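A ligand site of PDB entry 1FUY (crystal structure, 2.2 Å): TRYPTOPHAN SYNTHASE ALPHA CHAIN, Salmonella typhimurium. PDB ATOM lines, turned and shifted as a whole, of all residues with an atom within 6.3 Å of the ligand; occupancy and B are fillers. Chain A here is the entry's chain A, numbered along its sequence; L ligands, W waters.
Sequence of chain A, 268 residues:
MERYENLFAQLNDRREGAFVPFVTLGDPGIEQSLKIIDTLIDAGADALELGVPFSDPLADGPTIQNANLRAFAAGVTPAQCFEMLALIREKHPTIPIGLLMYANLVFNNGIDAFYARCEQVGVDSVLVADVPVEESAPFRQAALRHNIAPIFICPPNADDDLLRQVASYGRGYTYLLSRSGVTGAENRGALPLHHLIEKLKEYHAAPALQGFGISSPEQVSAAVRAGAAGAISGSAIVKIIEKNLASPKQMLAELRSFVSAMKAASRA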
ATOM      1  N   PHE A  22      -4.469  19.854   4.011  1.00  0.00           N
ATOM      2  CA  PHE A  22      -4.783  19.013   2.892  1.00  0.00           C
ATOM      3  C   PHE A  22      -3.801  19.391   1.776  1.00  0.00           C
ATOM      4  O   PHE A  22      -3.620  20.597   1.560  1.00  0.00           O
ATOM      5  CB  PHE A  22      -6.239  19.238   2.395  1.00  0.00           C
ATOM      6  CG  PHE A  22      -6.386  18.620   1.025  1.00  0.00           C
ATOM      7  CD1 PHE A  22      -5.986  19.307  -0.134  1.00  0.00           C
ATOM      8  CD2 PHE A  22      -6.860  17.337   0.841  1.00  0.00           C
ATOM      9  CE1 PHE A  22      -6.066  18.736  -1.386  1.00  0.00           C
ATOM     10  CE2 PHE A  22      -6.969  16.765  -0.397  1.00  0.00           C
ATOM     11  CZ  PHE A  22      -6.553  17.451  -1.527  1.00  0.00           C
ATOM     12  N   GLU A  49      -4.360  15.271   5.652  1.00  0.00           N
ATOM     13  CA  GLU A  49      -5.450  14.944   4.766  1.00  0.00           C
ATOM     14  C   GLU A  49      -4.822  14.994   3.349  1.00  0.00           C
ATOM     15  O   GLU A  49      -4.224  16.001   2.950  1.00  0.00           O
ATOM     16  CB  GLU A  49      -6.693  15.799   4.817  1.00  0.00           C
ATOM     17  CG  GLU A  49      -7.835  15.169   4.014  1.00  0.00           C
ATOM     18  CD  GLU A  49      -8.329  13.959   4.810  1.00  0.00           C
ATOM     19  OE1 GLU A  49      -8.165  13.843   6.051  1.00  0.00           O
ATOM     20  OE2 GLU A  49      -8.856  13.070   4.110  1.00  0.00           O
ATOM     21  N   ALA A  59     -15.758  17.500  -6.783  1.00  0.00           N
ATOM     22  CA  ALA A  59     -16.119  18.299  -5.592  1.00  0.00           C
ATOM     23  C   ALA A  59     -15.013  19.301  -5.264  1.00  0.00           C
ATOM     24  O   ALA A  59     -14.935  19.904  -4.188  1.00  0.00           O
ATOM     25  CB  ALA A  59     -16.449  17.437  -4.402  1.00  0.00           C
ATOM     26  N   ASP A  60     -14.119  19.574  -6.205  1.00  0.00           N
ATOM     27  CA  ASP A  60     -13.009  20.468  -6.048  1.00  0.00           C
ATOM     28  C   ASP A  60     -12.979  21.720  -6.930  1.00  0.00           C
ATOM     29  O   ASP A  60     -13.027  21.724  -8.163  1.00  0.00           O
ATOM     30  CB  ASP A  60     -11.721  19.670  -6.385  1.00  0.00           C
ATOM     31  CG  ASP A  60     -11.317  18.711  -5.279  1.00  0.00           C
ATOM     32  OD1 ASP A  60     -11.015  19.303  -4.211  1.00  0.00           O
ATOM     33  OD2 ASP A  60     -11.291  17.474  -5.462  1.00  0.00           O
ATOM     34  N   ILE A  64      -7.407  23.366  -6.315  1.00  0.00           N
ATOM     35  CA  ILE A  64      -7.115  21.922  -6.254  1.00  0.00           C
ATOM     36  C   ILE A  64      -7.243  21.249  -7.589  1.00  0.00           C
ATOM     37  O   ILE A  64      -6.449  20.326  -7.838  1.00  0.00           O
ATOM     38  CB  ILE A  64      -7.927  21.259  -5.116  1.00  0.00           C
ATOM     39  CG1 ILE A  64      -7.408  21.906  -3.818  1.00  0.00           C
ATOM     40  CG2 ILE A  64      -7.767  19.731  -5.130  1.00  0.00           C
ATOM     41  CD1 ILE A  64      -7.976  21.437  -2.521  1.00  0.00           C
ATOM     42  N   LEU A 100      -8.157  11.591   0.781  1.00  0.00           N
ATOM     43  CA  LEU A 100      -9.399  12.158   0.206  1.00  0.00           C
ATOM     44  C   LEU A 100      -9.530  11.460  -1.146  1.00  0.00           C
ATOM     45  O   LEU A 100      -8.626  11.712  -1.954  1.00  0.00           O
ATOM     46  CB  LEU A 100      -9.290  13.631  -0.133  1.00  0.00           C
ATOM     47  CG  LEU A 100     -10.522  14.360  -0.628  1.00  0.00           C
ATOM     48  CD1 LEU A 100     -10.842  14.032  -2.081  1.00  0.00           C
ATOM     49  CD2 LEU A 100     -11.693  14.182   0.287  1.00  0.00           C
ATOM     50  N   TYR A 102     -11.856   9.933  -4.706  1.00  0.00           N
ATOM     51  CA  TYR A 102     -13.086   9.957  -5.472  1.00  0.00           C
ATOM     52  C   TYR A 102     -13.443   8.477  -5.607  1.00  0.00           C
ATOM     53  O   TYR A 102     -12.510   7.695  -5.606  1.00  0.00           O
ATOM     54  CB  TYR A 102     -12.917  10.649  -6.855  1.00  0.00           C
ATOM     55  CG  TYR A 102     -12.985  12.137  -6.554  1.00  0.00           C
ATOM     56  CD1 TYR A 102     -14.214  12.787  -6.552  1.00  0.00           C
ATOM     57  CD2 TYR A 102     -11.820  12.876  -6.285  1.00  0.00           C
ATOM     58  CE1 TYR A 102     -14.330  14.143  -6.280  1.00  0.00           C
ATOM     59  CE2 TYR A 102     -11.948  14.251  -5.973  1.00  0.00           C
ATOM     60  CZ  TYR A 102     -13.208  14.853  -6.012  1.00  0.00           C
ATOM     61  OH  TYR A 102     -13.283  16.169  -5.791  1.00  0.00           O
ATOM     62  N   LEU A 127     -11.932   9.166   3.121  1.00  0.00           N
ATOM     63  CA  LEU A 127     -13.144   9.903   2.816  1.00  0.00           C
ATOM     64  C   LEU A 127     -13.261   9.759   1.274  1.00  0.00           C
ATOM     65  O   LEU A 127     -12.427  10.247   0.520  1.00  0.00           O
ATOM     66  CB  LEU A 127     -12.982  11.403   3.075  1.00  0.00           C
ATOM     67  CG  LEU A 127     -14.213  12.287   3.324  1.00  0.00           C
ATOM     68  CD1 LEU A 127     -13.749  13.710   3.726  1.00  0.00           C
ATOM     69  CD2 LEU A 127     -15.112  12.331   2.116  1.00  0.00           C
ATOM     70  N   ALA A 129     -15.267  11.275  -1.567  1.00  0.00           N
ATOM     71  CA  ALA A 129     -16.073  12.494  -1.778  1.00  0.00           C
ATOM     72  C   ALA A 129     -17.371  12.226  -2.512  1.00  0.00           C
ATOM     73  O   ALA A 129     -18.371  12.756  -2.018  1.00  0.00           O
ATOM     74  CB  ALA A 129     -15.113  13.469  -2.444  1.00  0.00           C
ATOM     75  N   ILE A 153     -19.103  13.138   5.352  1.00  0.00           N
ATOM     76  CA  ILE A 153     -19.253  14.582   5.344  1.00  0.00           C
ATOM     77  C   ILE A 153     -20.563  14.930   6.011  1.00  0.00           C
ATOM     78  O   ILE A 153     -21.586  14.297   5.741  1.00  0.00           O
ATOM     79  CB  ILE A 153     -19.218  15.103   3.908  1.00  0.00           C
ATOM     80  CG1 ILE A 153     -17.793  14.901   3.370  1.00  0.00           C
ATOM     81  CG2 ILE A 153     -19.558  16.584   3.727  1.00  0.00           C
ATOM     82  CD1 ILE A 153     -17.575  15.271   1.918  1.00  0.00           C
ATOM     83  N   TYR A 175     -16.415  14.774   9.166  1.00  0.00           N
ATOM     84  CA  TYR A 175     -15.996  15.884   8.331  1.00  0.00           C
ATOM     85  C   TYR A 175     -17.176  16.846   8.250  1.00  0.00           C
ATOM     86  O   TYR A 175     -18.197  16.599   7.630  1.00  0.00           O
ATOM     87  CB  TYR A 175     -15.473  15.486   6.980  1.00  0.00           C
ATOM     88  CG  TYR A 175     -14.875  16.599   6.162  1.00  0.00           C
ATOM     89  CD1 TYR A 175     -15.758  17.489   5.594  1.00  0.00           C
ATOM     90  CD2 TYR A 175     -13.557  16.714   5.846  1.00  0.00           C
ATOM     91  CE1 TYR A 175     -15.342  18.545   4.796  1.00  0.00           C
ATOM     92  CE2 TYR A 175     -13.072  17.747   5.072  1.00  0.00           C
ATOM     93  CZ  TYR A 175     -13.977  18.664   4.574  1.00  0.00           C
ATOM     94  OH  TYR A 175     -13.624  19.713   3.776  1.00  0.00           O
ATOM     95  N   LEU A 177     -18.735  20.056   6.796  1.00  0.00           N
ATOM     96  CA  LEU A 177     -18.704  20.931   5.633  1.00  0.00           C
ATOM     97  C   LEU A 177     -19.169  22.325   6.017  1.00  0.00           C
ATOM     98  O   LEU A 177     -20.231  22.568   6.583  1.00  0.00           O
ATOM     99  CB  LEU A 177     -19.580  20.280   4.544  1.00  0.00           C
ATOM    100  CG  LEU A 177     -19.263  20.719   3.131  1.00  0.00           C
ATOM    101  CD1 LEU A 177     -17.799  20.493   2.815  1.00  0.00           C
ATOM    102  CD2 LEU A 177     -20.131  19.979   2.123  1.00  0.00           C
ATOM    103  N   ARG A 179     -19.850  25.018   4.093  1.00  0.00           N
ATOM    104  CA  ARG A 179     -20.783  25.556   3.146  1.00  0.00           C
ATOM    105  C   ARG A 179     -20.998  24.621   1.924  1.00  0.00           C
ATOM    106  O   ARG A 179     -20.286  23.632   1.734  1.00  0.00           O
ATOM    107  CB  ARG A 179     -20.236  26.853   2.486  1.00  0.00           C
ATOM    108  CG  ARG A 179     -18.896  26.485   1.817  1.00  0.00           C
ATOM    109  CD  ARG A 179     -18.399  27.665   1.025  1.00  0.00           C
ATOM    110  NE  ARG A 179     -17.016  27.561   0.614  1.00  0.00           N
ATOM    111  CZ  ARG A 179     -16.564  26.730  -0.332  1.00  0.00           C
ATOM    112  NH1 ARG A 179     -17.425  25.898  -0.914  1.00  0.00           N
ATOM    113  NH2 ARG A 179     -15.271  26.733  -0.683  1.00  0.00           N
ATOM    114  N   VAL A 182     -18.013  23.894  -3.699  1.00  0.00           N
ATOM    115  CA  VAL A 182     -16.827  23.069  -3.746  1.00  0.00           C
ATOM    116  C   VAL A 182     -15.612  23.564  -2.987  1.00  0.00           C
ATOM    117  O   VAL A 182     -15.558  24.706  -2.590  1.00  0.00           O
ATOM    118  CB  VAL A 182     -16.305  22.883  -5.213  1.00  0.00           C
ATOM    119  CG1 VAL A 182     -17.431  22.332  -6.098  1.00  0.00           C
ATOM    120  CG2 VAL A 182     -15.691  24.138  -5.786  1.00  0.00           C
ATOM    121  N   THR A 183     -14.570  22.749  -2.895  1.00  0.00           N
ATOM    122  CA  THR A 183     -13.396  23.246  -2.172  1.00  0.00           C
ATOM    123  C   THR A 183     -12.957  24.585  -2.782  1.00  0.00           C
ATOM    124  O   THR A 183     -13.160  24.751  -3.994  1.00  0.00           O
ATOM    125  CB  THR A 183     -12.205  22.301  -2.236  1.00  0.00           C
ATOM    126  OG1 THR A 183     -11.854  22.131  -3.632  1.00  0.00           O
ATOM    127  CG2 THR A 183     -12.535  20.978  -1.601  1.00  0.00           C
ATOM    128  N   GLY A 184     -12.356  25.468  -1.990  1.00  0.00           N
ATOM    129  CA  GLY A 184     -11.943  26.742  -2.589  1.00  0.00           C
ATOM    130  C   GLY A 184     -11.831  27.810  -1.501  1.00  0.00           C
ATOM    131  O   GLY A 184     -12.800  28.261  -0.900  1.00  0.00           O
ATOM    132  N   ALA A 185     -10.596  28.285  -1.412  1.00  0.00           N
ATOM    133  CA  ALA A 185     -10.135  29.258  -0.450  1.00  0.00           C
ATOM    134  C   ALA A 185     -10.875  30.575  -0.610  1.00  0.00           C
ATOM    135  O   ALA A 185     -10.861  31.423   0.274  1.00  0.00           O
ATOM    136  CB  ALA A 185      -8.643  29.526  -0.594  1.00  0.00           C
ATOM    137  N   GLY A 211     -14.173  21.979   7.611  1.00  0.00           N
ATOM    138  CA  GLY A 211     -13.438  22.253   6.407  1.00  0.00           C
ATOM    139  C   GLY A 211     -14.206  22.796   5.225  1.00  0.00           C
ATOM    140  O   GLY A 211     -15.441  22.781   5.133  1.00  0.00           O
ATOM    141  N   PHE A 212     -13.518  23.258   4.208  1.00  0.00           N
ATOM    142  CA  PHE A 212     -14.094  23.964   3.073  1.00  0.00           C
ATOM    143  C   PHE A 212     -14.015  25.457   3.466  1.00  0.00           C
ATOM    144  O   PHE A 212     -14.522  25.843   4.512  1.00  0.00           O
ATOM    145  CB  PHE A 212     -15.518  23.702   2.629  1.00  0.00           C
ATOM    146  CG  PHE A 212     -15.620  22.609   1.593  1.00  0.00           C
ATOM    147  CD1 PHE A 212     -14.662  21.596   1.547  1.00  0.00           C
ATOM    148  CD2 PHE A 212     -16.644  22.572   0.665  1.00  0.00           C
ATOM    149  CE1 PHE A 212     -14.752  20.590   0.601  1.00  0.00           C
ATOM    150  CE2 PHE A 212     -16.763  21.553  -0.287  1.00  0.00           C
ATOM    151  CZ  PHE A 212     -15.780  20.583  -0.341  1.00  0.00           C
ATOM    152  N   GLY A 213     -13.202  26.176   2.717  1.00  0.00           N
ATOM    153  CA  GLY A 213     -13.062  27.588   2.950  1.00  0.00           C
ATOM    154  C   GLY A 213     -12.178  28.015   4.094  1.00  0.00           C
ATOM    155  O   GLY A 213     -11.815  29.202   4.050  1.00  0.00           O
ATOM    156  N   ILE A 214     -11.805  27.198   5.066  1.00  0.00           N
ATOM    157  CA  ILE A 214     -10.944  27.655   6.159  1.00  0.00           C
ATOM    158  C   ILE A 214      -9.594  28.123   5.644  1.00  0.00           C
ATOM    159  O   ILE A 214      -8.784  27.264   5.264  1.00  0.00           O
ATOM    160  CB  ILE A 214     -10.691  26.513   7.154  1.00  0.00           C
ATOM    161  CG1 ILE A 214     -11.991  25.972   7.711  1.00  0.00           C
ATOM    162  CG2 ILE A 214      -9.690  26.943   8.222  1.00  0.00           C
ATOM    163  CD1 ILE A 214     -12.563  26.679   8.921  1.00  0.00           C
ATOM    164  N   SER A 215      -9.237  29.410   5.680  1.00  0.00           N
ATOM    165  CA  SER A 215      -8.021  29.948   5.144  1.00  0.00           C
ATOM    166  C   SER A 215      -7.126  30.823   6.011  1.00  0.00           C
ATOM    167  O   SER A 215      -6.029  31.207   5.610  1.00  0.00           O
ATOM    168  CB  SER A 215      -8.487  30.843   3.962  1.00  0.00           C
ATOM    169  OG  SER A 215      -7.457  30.868   3.003  1.00  0.00           O
ATOM    170  N   ILE A 232      -9.627  21.607   8.973  1.00  0.00           N
ATOM    171  CA  ILE A 232      -8.793  21.119   7.846  1.00  0.00           C
ATOM    172  C   ILE A 232      -8.626  22.321   6.931  1.00  0.00           C
ATOM    173  O   ILE A 232      -9.642  23.001   6.780  1.00  0.00           O
ATOM    174  CB  ILE A 232      -9.510  20.000   7.065  1.00  0.00           C
ATOM    175  CG1 ILE A 232      -9.484  18.678   7.847  1.00  0.00           C
ATOM    176  CG2 ILE A 232      -9.019  19.825   5.641  1.00  0.00           C
ATOM    177  CD1 ILE A 232     -10.693  17.844   7.412  1.00  0.00           C
ATOM    178  N   SER A 233      -7.537  22.497   6.231  1.00  0.00           N
ATOM    179  CA  SER A 233      -7.428  23.582   5.267  1.00  0.00           C
ATOM    180  C   SER A 233      -6.651  23.120   4.063  1.00  0.00           C
ATOM    181  O   SER A 233      -5.545  22.609   4.203  1.00  0.00           O
ATOM    182  CB  SER A 233      -6.724  24.737   5.994  1.00  0.00           C
ATOM    183  OG  SER A 233      -5.980  25.479   5.039  1.00  0.00           O
ATOM    184  N   GLY A 234      -7.183  23.304   2.841  1.00  0.00           N
ATOM    185  CA  GLY A 234      -6.472  22.769   1.654  1.00  0.00           C
ATOM    186  C   GLY A 234      -6.052  23.825   0.633  1.00  0.00           C
ATOM    187  O   GLY A 234      -4.865  24.016   0.385  1.00  0.00           O
ATOM    188  N   SER A 235      -7.033  24.541   0.088  1.00  0.00           N
ATOM    189  CA  SER A 235      -6.807  25.519  -0.970  1.00  0.00           C
ATOM    190  C   SER A 235      -5.805  26.566  -0.564  1.00  0.00           C
ATOM    191  O   SER A 235      -4.822  26.783  -1.265  1.00  0.00           O
ATOM    192  CB  SER A 235      -8.096  26.166  -1.488  1.00  0.00           C
ATOM    193  OG  SER A 235      -8.830  25.112  -2.142  1.00  0.00           O
ATOM    194  N   ALA A 236      -5.950  27.079   0.654  1.00  0.00           N
ATOM    195  CA  ALA A 236      -4.989  28.039   1.177  1.00  0.00           C
ATOM    196  C   ALA A 236      -3.632  27.397   1.290  1.00  0.00           C
ATOM    197  O   ALA A 236      -2.717  28.187   0.966  1.00  0.00           O
ATOM    198  CB  ALA A 236      -5.433  28.708   2.456  1.00  0.00           C
HETATM  199  C1  LIG L   1     -10.641  18.646   0.508  1.00  0.00           C
HETATM  200  C2  LIG L   1     -11.910  18.115   0.096  1.00  0.00           C
HETATM  201  C3  LIG L   1     -11.792  17.897  -1.295  1.00  0.00           C
HETATM  202  C4  LIG L   1     -13.105  17.800   0.735  1.00  0.00           C
HETATM  203  C5  LIG L   1      -9.864  18.736  -0.598  1.00  0.00           C
HETATM  204  N1  LIG L   1     -10.546  18.292  -1.706  1.00  0.00           N
HETATM  205  C6  LIG L   1     -12.825  17.405  -2.077  1.00  0.00           C
HETATM  206  C7  LIG L   1     -14.139  17.273  -0.074  1.00  0.00           C
HETATM  207  C8  LIG L   1     -13.994  17.079  -1.440  1.00  0.00           C
HETATM  208  F1  LIG L   1     -15.305  16.941   0.442  1.00  0.00           F
HETATM  209  C9  LIG L   1     -10.278  19.054   1.906  1.00  0.00           C
HETATM  210  C10 LIG L   1     -11.021  20.415   2.137  1.00  0.00           C
HETATM  211  C11 LIG L   1     -10.606  21.478   1.105  1.00  0.00           C
HETATM  212  P1  LIG L   1     -10.664  24.061   0.961  1.00  0.00           P
HETATM  213  O1  LIG L   1      -9.856  23.788  -0.229  1.00  0.00           O
HETATM  214  O2  LIG L   1      -9.822  24.395   2.142  1.00  0.00           O
HETATM  215  O3  LIG L   1     -11.876  24.919   0.825  1.00  0.00           O
HETATM  216  O4  LIG L   1     -11.326  22.678   1.392  1.00  0.00           O
HETATM  217  O   HOH W   1     -10.918  24.400   4.457  1.00  0.00           O
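The backbone NH (N) of Ser 235 lies close to an oxygen (O1) of the ligand. The side-chain hydroxyl (OG) of Ser 235 sits close to an oxygen (O1) of the ligand. N of Gly 213 sits close to O3 of the ligand, at 2.6 Å. A nitrogen (N1) of the ligand lies close to the side-chain carboxylate of Asp 60 (2.7 Å). N of Gly 184 sits close to O3 of the ligand. An oxygen (O2) of the ligand sits close to the backbone NH of Gly 234 (2.9 Å).
The side-chain carboxylate (OD1) of Asp 60 is in hydrogen-bond range of the side-chain hydroxyl (OG1) of Thr 183 (3.0 Å). OD2 of Asp 60 sits at hydrogen-bond distance from OH of Tyr 102. The guanidinium group of Arg 179 sits at hydrogen-bond distance from the backbone carbonyl oxygen of Gly 184. The backbone NH of Thr 183 sits at hydrogen-bond distance from the backbone carbonyl oxygen of Ala 59 (3.1 Å). O of Ser 233 sits at hydrogen-bond distance from N of Phe 22, at 3.0 Å. The backbone NH of Ala 59 sits at hydrogen-bond distance from the side-chain hydroxyl of Tyr 102, 3.0 Å away. OG of Ser 233 is in hydrogen-bond range of O of Ile 214.
Merely in contact with the ligand: Phe 22, Ala 59, Ile 64, Leu 100, Tyr 102, Ala 129, Ile 153, Tyr 175, Thr 183, Phe 212 and Ser 233. Hydrophobic or aromatic side chains that line the ligand: Phe 22, Ala 59, Ile 64, Leu 100, Ala 129, Ile 153 and Phe 212. Along chain A the residues within 4 Å of the ligand span positions 22 to 235. The nearest printed residue that does not touch the ligand is Ile 232 (4.02 Å).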
